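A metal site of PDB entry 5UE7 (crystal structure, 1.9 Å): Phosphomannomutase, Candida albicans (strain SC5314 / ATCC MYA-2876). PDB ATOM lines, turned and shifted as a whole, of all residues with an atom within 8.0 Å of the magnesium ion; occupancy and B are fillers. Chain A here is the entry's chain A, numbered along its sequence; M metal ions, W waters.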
ATOM      1  N   PHE A  15       4.056  27.675  28.194  1.00  0.00           N
ATOM      2  CA  PHE A  15       4.952  26.556  27.944  1.00  0.00           C
ATOM      3  C   PHE A  15       4.344  25.629  26.916  1.00  0.00           C
ATOM      4  O   PHE A  15       3.214  25.170  27.093  1.00  0.00           O
ATOM      5  CB  PHE A  15       5.224  25.746  29.199  1.00  0.00           C
ATOM      6  CG  PHE A  15       5.878  26.523  30.289  1.00  0.00           C
ATOM      7  CD1 PHE A  15       5.106  27.196  31.215  1.00  0.00           C
ATOM      8  CD2 PHE A  15       7.254  26.560  30.388  1.00  0.00           C
ATOM      9  CE1 PHE A  15       5.714  27.912  32.229  1.00  0.00           C
ATOM     10  CE2 PHE A  15       7.863  27.277  31.402  1.00  0.00           C
ATOM     11  CZ  PHE A  15       7.104  27.947  32.323  1.00  0.00           C
ATOM     12  N   ASP A  16       5.103  25.296  25.884  1.00  0.00           N
ATOM     13  CA  ASP A  16       4.829  24.049  25.197  1.00  0.00           C
ATOM     14  C   ASP A  16       4.921  22.911  26.192  1.00  0.00           C
ATOM     15  O   ASP A  16       5.666  22.979  27.186  1.00  0.00           O
ATOM     16  CB  ASP A  16       5.809  23.850  24.041  1.00  0.00           C
ATOM     17  CG  ASP A  16       5.758  22.445  23.487  1.00  0.00           C
ATOM     18  OD1 ASP A  16       4.715  22.058  22.927  1.00  0.00           O
ATOM     19  OD2 ASP A  16       6.776  21.737  23.615  1.00  0.00           O
ATOM     20  N   VAL A  17       4.139  21.858  25.982  1.00  0.00           N
ATOM     21  CA  VAL A  17       4.119  20.762  26.950  1.00  0.00           C
ATOM     22  C   VAL A  17       5.222  19.763  26.624  1.00  0.00           C
ATOM     23  O   VAL A  17       6.227  19.668  27.336  1.00  0.00           O
ATOM     24  CB  VAL A  17       2.753  20.064  27.007  1.00  0.00           C
ATOM     25  CG1 VAL A  17       2.806  18.906  27.994  1.00  0.00           C
ATOM     26  CG2 VAL A  17       1.663  21.043  27.412  1.00  0.00           C
ATOM     27  N   ASP A  18       5.034  19.000  25.540  1.00  0.00           N
ATOM     28  CA  ASP A  18       5.930  17.890  25.227  1.00  0.00           C
ATOM     29  C   ASP A  18       7.333  18.382  24.916  1.00  0.00           C
ATOM     30  O   ASP A  18       7.536  19.173  23.993  1.00  0.00           O
ATOM     31  CB  ASP A  18       5.377  17.092  24.053  1.00  0.00           C
ATOM     32  CG  ASP A  18       6.224  15.876  23.757  1.00  0.00           C
ATOM     33  OD1 ASP A  18       6.095  14.877  24.498  1.00  0.00           O
ATOM     34  OD2 ASP A  18       7.032  15.929  22.805  1.00  0.00           O
ATOM     35  N   GLY A  19       8.313  17.863  25.664  1.00  0.00           N
ATOM     36  CA  GLY A  19       9.697  18.198  25.429  1.00  0.00           C
ATOM     37  C   GLY A  19      10.140  19.510  26.037  1.00  0.00           C
ATOM     38  O   GLY A  19      11.341  19.825  25.978  1.00  0.00           O
ATOM     39  N   THR A  20       9.228  20.283  26.608  1.00  0.00           N
ATOM     40  CA  THR A  20       9.547  21.542  27.268  1.00  0.00           C
ATOM     41  C   THR A  20       9.280  21.470  28.764  1.00  0.00           C
ATOM     42  O   THR A  20      10.166  21.771  29.558  1.00  0.00           O
ATOM     43  CB  THR A  20       8.739  22.686  26.636  1.00  0.00           C
ATOM     44  OG1 THR A  20       9.021  22.758  25.231  1.00  0.00           O
ATOM     45  CG2 THR A  20       9.087  24.025  27.284  1.00  0.00           C
ATOM     46  N   LEU A  21       8.074  21.074  29.161  1.00  0.00           N
ATOM     47  CA  LEU A  21       7.749  20.845  30.564  1.00  0.00           C
ATOM     48  C   LEU A  21       8.015  19.412  30.984  1.00  0.00           C
ATOM     49  O   LEU A  21       8.246  19.145  32.168  1.00  0.00           O
ATOM     50  CB  LEU A  21       6.285  21.174  30.832  1.00  0.00           C
ATOM     51  CG  LEU A  21       5.887  22.654  30.900  1.00  0.00           C
ATOM     52  CD1 LEU A  21       4.397  22.787  31.134  1.00  0.00           C
ATOM     53  CD2 LEU A  21       6.685  23.360  31.980  1.00  0.00           C
ATOM     54  N   THR A  22       7.951  18.479  30.047  1.00  0.00           N
ATOM     55  CA  THR A  22       8.180  17.060  30.257  1.00  0.00           C
ATOM     56  C   THR A  22       9.330  16.603  29.372  1.00  0.00           C
ATOM     57  O   THR A  22       9.724  17.306  28.429  1.00  0.00           O
ATOM     58  CB  THR A  22       6.929  16.245  29.899  1.00  0.00           C
ATOM     59  OG1 THR A  22       6.903  16.013  28.481  1.00  0.00           O
ATOM     60  CG2 THR A  22       5.669  16.980  30.309  1.00  0.00           C
ATOM     61  N   PRO A  23       9.902  15.423  29.639  1.00  0.00           N
ATOM     62  CA  PRO A  23      10.843  14.835  28.679  1.00  0.00           C
ATOM     63  C   PRO A  23      10.204  14.578  27.322  1.00  0.00           C
ATOM     64  O   PRO A  23       9.007  14.827  27.143  1.00  0.00           O
ATOM     65  CB  PRO A  23      11.257  13.520  29.358  1.00  0.00           C
ATOM     66  CG  PRO A  23      11.110  13.807  30.817  1.00  0.00           C
ATOM     67  CD  PRO A  23       9.908  14.711  30.933  1.00  0.00           C
ATOM     68  N   ALA A  24      11.000  14.052  26.393  1.00  0.00           N
ATOM     69  CA  ALA A  24      10.591  13.967  24.988  1.00  0.00           C
ATOM     70  C   ALA A  24       9.229  13.304  24.810  1.00  0.00           C
ATOM     71  O   ALA A  24       8.458  13.690  23.923  1.00  0.00           O
ATOM     72  CB  ALA A  24      11.647  13.210  24.191  1.00  0.00           C
ATOM     73  N   VAL A  48       0.452  25.379  26.435  1.00  0.00           N
ATOM     74  CA  VAL A  48      -0.243  25.205  25.162  1.00  0.00           C
ATOM     75  C   VAL A  48       0.363  24.006  24.443  1.00  0.00           C
ATOM     76  O   VAL A  48       1.595  23.902  24.323  1.00  0.00           O
ATOM     77  CB  VAL A  48      -0.206  26.455  24.270  1.00  0.00           C
ATOM     78  CG1 VAL A  48       1.233  26.972  24.089  1.00  0.00           C
ATOM     79  CG2 VAL A  48      -0.883  26.192  22.937  1.00  0.00           C
ATOM     80  N   GLY A  49      -0.486  23.092  23.995  1.00  0.00           N
ATOM     81  CA  GLY A  49      -0.049  21.933  23.260  1.00  0.00           C
ATOM     82  C   GLY A  49      -1.054  21.602  22.175  1.00  0.00           C
ATOM     83  O   GLY A  49      -2.225  21.984  22.250  1.00  0.00           O
ATOM     84  N   GLN A  59       0.618  13.630  30.407  1.00  0.00           N
ATOM     85  CA  GLN A  59       1.904  14.313  30.542  1.00  0.00           C
ATOM     86  C   GLN A  59       1.988  15.190  31.787  1.00  0.00           C
ATOM     87  O   GLN A  59       3.026  15.197  32.466  1.00  0.00           O
ATOM     88  CB  GLN A  59       2.177  15.168  29.297  1.00  0.00           C
ATOM     89  CG  GLN A  59       2.249  14.401  27.993  1.00  0.00           C
ATOM     90  CD  GLN A  59       2.108  15.310  26.775  1.00  0.00           C
ATOM     91  OE1 GLN A  59       1.076  15.957  26.590  1.00  0.00           O
ATOM     92  NE2 GLN A  59       3.142  15.343  25.949  1.00  0.00           N
ATOM     93  N   LYS A 193      -0.144  27.147  17.363  1.00  0.00           N
ATOM     94  CA  LYS A 193      -0.043  27.522  18.770  1.00  0.00           C
ATOM     95  C   LYS A 193      -0.370  28.995  19.014  1.00  0.00           C
ATOM     96  O   LYS A 193      -0.838  29.345  20.098  1.00  0.00           O
ATOM     97  CB  LYS A 193       1.365  27.207  19.290  1.00  0.00           C
ATOM     98  CG  LYS A 193       1.593  25.747  19.689  1.00  0.00           C
ATOM     99  CD  LYS A 193       2.748  25.653  20.688  1.00  0.00           C
ATOM    100  CE  LYS A 193       2.935  24.243  21.227  1.00  0.00           C
ATOM    101  NZ  LYS A 193       3.523  23.311  20.223  1.00  0.00           N
ATOM    102  N   PHE A 210       7.234  32.686  26.187  1.00  0.00           N
ATOM    103  CA  PHE A 210       6.925  31.355  25.686  1.00  0.00           C
ATOM    104  C   PHE A 210       8.186  30.506  25.683  1.00  0.00           C
ATOM    105  O   PHE A 210       9.245  30.960  25.221  1.00  0.00           O
ATOM    106  CB  PHE A 210       6.304  31.378  24.279  1.00  0.00           C
ATOM    107  CG  PHE A 210       6.278  30.006  23.633  1.00  0.00           C
ATOM    108  CD1 PHE A 210       5.200  29.164  23.863  1.00  0.00           C
ATOM    109  CD2 PHE A 210       7.237  29.616  22.722  1.00  0.00           C
ATOM    110  CE1 PHE A 210       5.133  27.916  23.279  1.00  0.00           C
ATOM    111  CE2 PHE A 210       7.167  28.363  22.117  1.00  0.00           C
ATOM    112  CZ  PHE A 210       6.124  27.525  22.388  1.00  0.00           C
ATOM    113  N   PHE A 211       8.058  29.281  26.172  1.00  0.00           N
ATOM    114  CA  PHE A 211       9.117  28.283  26.196  1.00  0.00           C
ATOM    115  C   PHE A 211       8.687  27.136  25.301  1.00  0.00           C
ATOM    116  O   PHE A 211       7.574  26.631  25.433  1.00  0.00           O
ATOM    117  CB  PHE A 211       9.349  27.762  27.631  1.00  0.00           C
ATOM    118  CG  PHE A 211      10.094  28.718  28.523  1.00  0.00           C
ATOM    119  CD1 PHE A 211       9.473  29.854  29.014  1.00  0.00           C
ATOM    120  CD2 PHE A 211      11.418  28.471  28.879  1.00  0.00           C
ATOM    121  CE1 PHE A 211      10.157  30.740  29.835  1.00  0.00           C
ATOM    122  CE2 PHE A 211      12.103  29.356  29.699  1.00  0.00           C
ATOM    123  CZ  PHE A 211      11.482  30.499  30.169  1.00  0.00           C
ATOM    124  N   GLY A 212       9.562  26.723  24.387  1.00  0.00           N
ATOM    125  CA  GLY A 212       9.247  25.599  23.514  1.00  0.00           C
ATOM    126  C   GLY A 212      10.490  24.943  22.981  1.00  0.00           C
ATOM    127  O   GLY A 212      11.518  25.587  22.757  1.00  0.00           O
ATOM    128  N   ASP A 213      10.393  23.636  22.736  1.00  0.00           N
ATOM    129  CA  ASP A 213      11.537  22.848  22.321  1.00  0.00           C
ATOM    130  C   ASP A 213      11.640  22.660  20.815  1.00  0.00           C
ATOM    131  O   ASP A 213      12.620  22.071  20.347  1.00  0.00           O
ATOM    132  CB  ASP A 213      11.521  21.467  22.996  1.00  0.00           C
ATOM    133  CG  ASP A 213      10.354  20.591  22.534  1.00  0.00           C
ATOM    134  OD1 ASP A 213       9.246  21.132  22.356  1.00  0.00           O
ATOM    135  OD2 ASP A 213      10.558  19.371  22.367  1.00  0.00           O
ATOM    136  N   LYS A 214      10.682  23.146  20.023  1.00  0.00           N
ATOM    137  CA  LYS A 214      10.706  22.990  18.572  1.00  0.00           C
ATOM    138  C   LYS A 214      10.363  24.330  17.902  1.00  0.00           C
ATOM    139  O   LYS A 214       9.444  24.444  17.105  1.00  0.00           O
ATOM    140  CB  LYS A 214       9.767  21.871  18.113  1.00  0.00           C
ATOM    141  CG  LYS A 214      10.004  20.504  18.789  1.00  0.00           C
ATOM    142  CD  LYS A 214      10.977  19.606  18.018  1.00  0.00           C
ATOM    143  CE  LYS A 214      11.294  18.312  18.790  1.00  0.00           C
ATOM    144  NZ  LYS A 214      12.271  17.418  18.083  1.00  0.00           N
ATOM    145  N   SER A 215      11.156  25.356  18.245  1.00  0.00           N
ATOM    146  CA  SER A 215      11.008  26.712  17.717  1.00  0.00           C
ATOM    147  C   SER A 215      11.673  26.905  16.362  1.00  0.00           C
ATOM    148  O   SER A 215      11.674  28.030  15.846  1.00  0.00           O
ATOM    149  CB  SER A 215      11.626  27.726  18.686  1.00  0.00           C
ATOM    150  OG  SER A 215      12.874  27.275  19.155  1.00  0.00           O
ATOM    151  N   ASN A 220       6.500  22.965  15.651  1.00  0.00           N
ATOM    152  CA  ASN A 220       5.180  23.447  16.033  1.00  0.00           C
ATOM    153  C   ASN A 220       5.234  24.592  17.041  1.00  0.00           C
ATOM    154  O   ASN A 220       4.173  25.092  17.454  1.00  0.00           O
ATOM    155  CB  ASN A 220       4.322  22.297  16.585  1.00  0.00           C
ATOM    156  CG  ASN A 220       4.963  21.570  17.762  1.00  0.00           C
ATOM    157  OD1 ASN A 220       5.794  22.119  18.476  1.00  0.00           O
ATOM    158  ND2 ASN A 220       4.573  20.320  17.949  1.00  0.00           N
ATOM    159  N   ASP A 221       6.428  25.020  17.450  1.00  0.00           N
ATOM    160  CA  ASP A 221       6.606  26.221  18.255  1.00  0.00           C
ATOM    161  C   ASP A 221       7.060  27.422  17.434  1.00  0.00           C
ATOM    162  O   ASP A 221       7.167  28.523  17.985  1.00  0.00           O
ATOM    163  CB  ASP A 221       7.617  25.954  19.376  1.00  0.00           C
ATOM    164  CG  ASP A 221       7.189  24.824  20.282  1.00  0.00           C
ATOM    165  OD1 ASP A 221       5.986  24.707  20.570  1.00  0.00           O
ATOM    166  OD2 ASP A 221       8.066  24.040  20.715  1.00  0.00           O
ATOM    167  N   VAL A 235      14.330  25.897  24.243  1.00  0.00           N
ATOM    168  CA  VAL A 235      14.899  24.932  25.183  1.00  0.00           C
ATOM    169  C   VAL A 235      15.075  23.601  24.475  1.00  0.00           C
ATOM    170  O   VAL A 235      14.552  23.368  23.388  1.00  0.00           O
ATOM    171  CB  VAL A 235      14.018  24.757  26.440  1.00  0.00           C
ATOM    172  CG1 VAL A 235      13.970  26.040  27.255  1.00  0.00           C
ATOM    173  CG2 VAL A 235      12.621  24.303  26.041  1.00  0.00           C
HETATM  174 MG    MG M   1       7.351  20.293  22.287  1.00  0.00          MG
HETATM  175  O   HOH W   1       5.544  19.652  21.927  1.00  0.00           O
HETATM  176  O   HOH W   2       7.244  21.666  20.786  1.00  0.00           O
HETATM  177  O   HOH W   3       8.140  18.303  21.589  1.00  0.00           O
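The side-chain amide nitrogen (NE2) of Gln 59 sits at hydrogen-bond distance from the side-chain carboxylate (OD1) of Asp 18 (3.3 Å).
The side-chain hydroxyl (OG1) of Thr 20 sits at hydrogen-bond distance from the backbone NH (N) of Asp 213 (3.0 Å).
The backbone NH (N) of Asp 213 sits at hydrogen-bond distance from the side-chain carboxylate (OD2) of Asp 221, 3.1 Å away.
OD2 of Asp 16 sits close to OG1 of Thr 20 (2.9 Å).
OD1 of Asp 16 is in salt-bridge range of NZ of Lys 193 (3.2 Å).
The side-chain carboxylate (OD1) of Asp 18 lies close to the backbone carbonyl oxygen (O) of Ala 24 (2.7 Å).
O of Phe 211 is in hydrogen-bond range of N of Asp 16, at 2.8 Å.
Water W3 bridges the side-chain carboxylate of Asp 213 and the side-chain carboxylate of Asp 18.
The magnesium ion is bound by water W1, water W2, OD2 of Asp 16, O of Asp 18, OD1 of Asp 213 and water W3.
The magnesium ion has six donor atoms within binding distance.
Of the 23 residues printed, 3 come within 4 Å of the magnesium ion.
The nearest printed residue that does not touch the magnesium ion is Asp 221 (4.1 Å).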
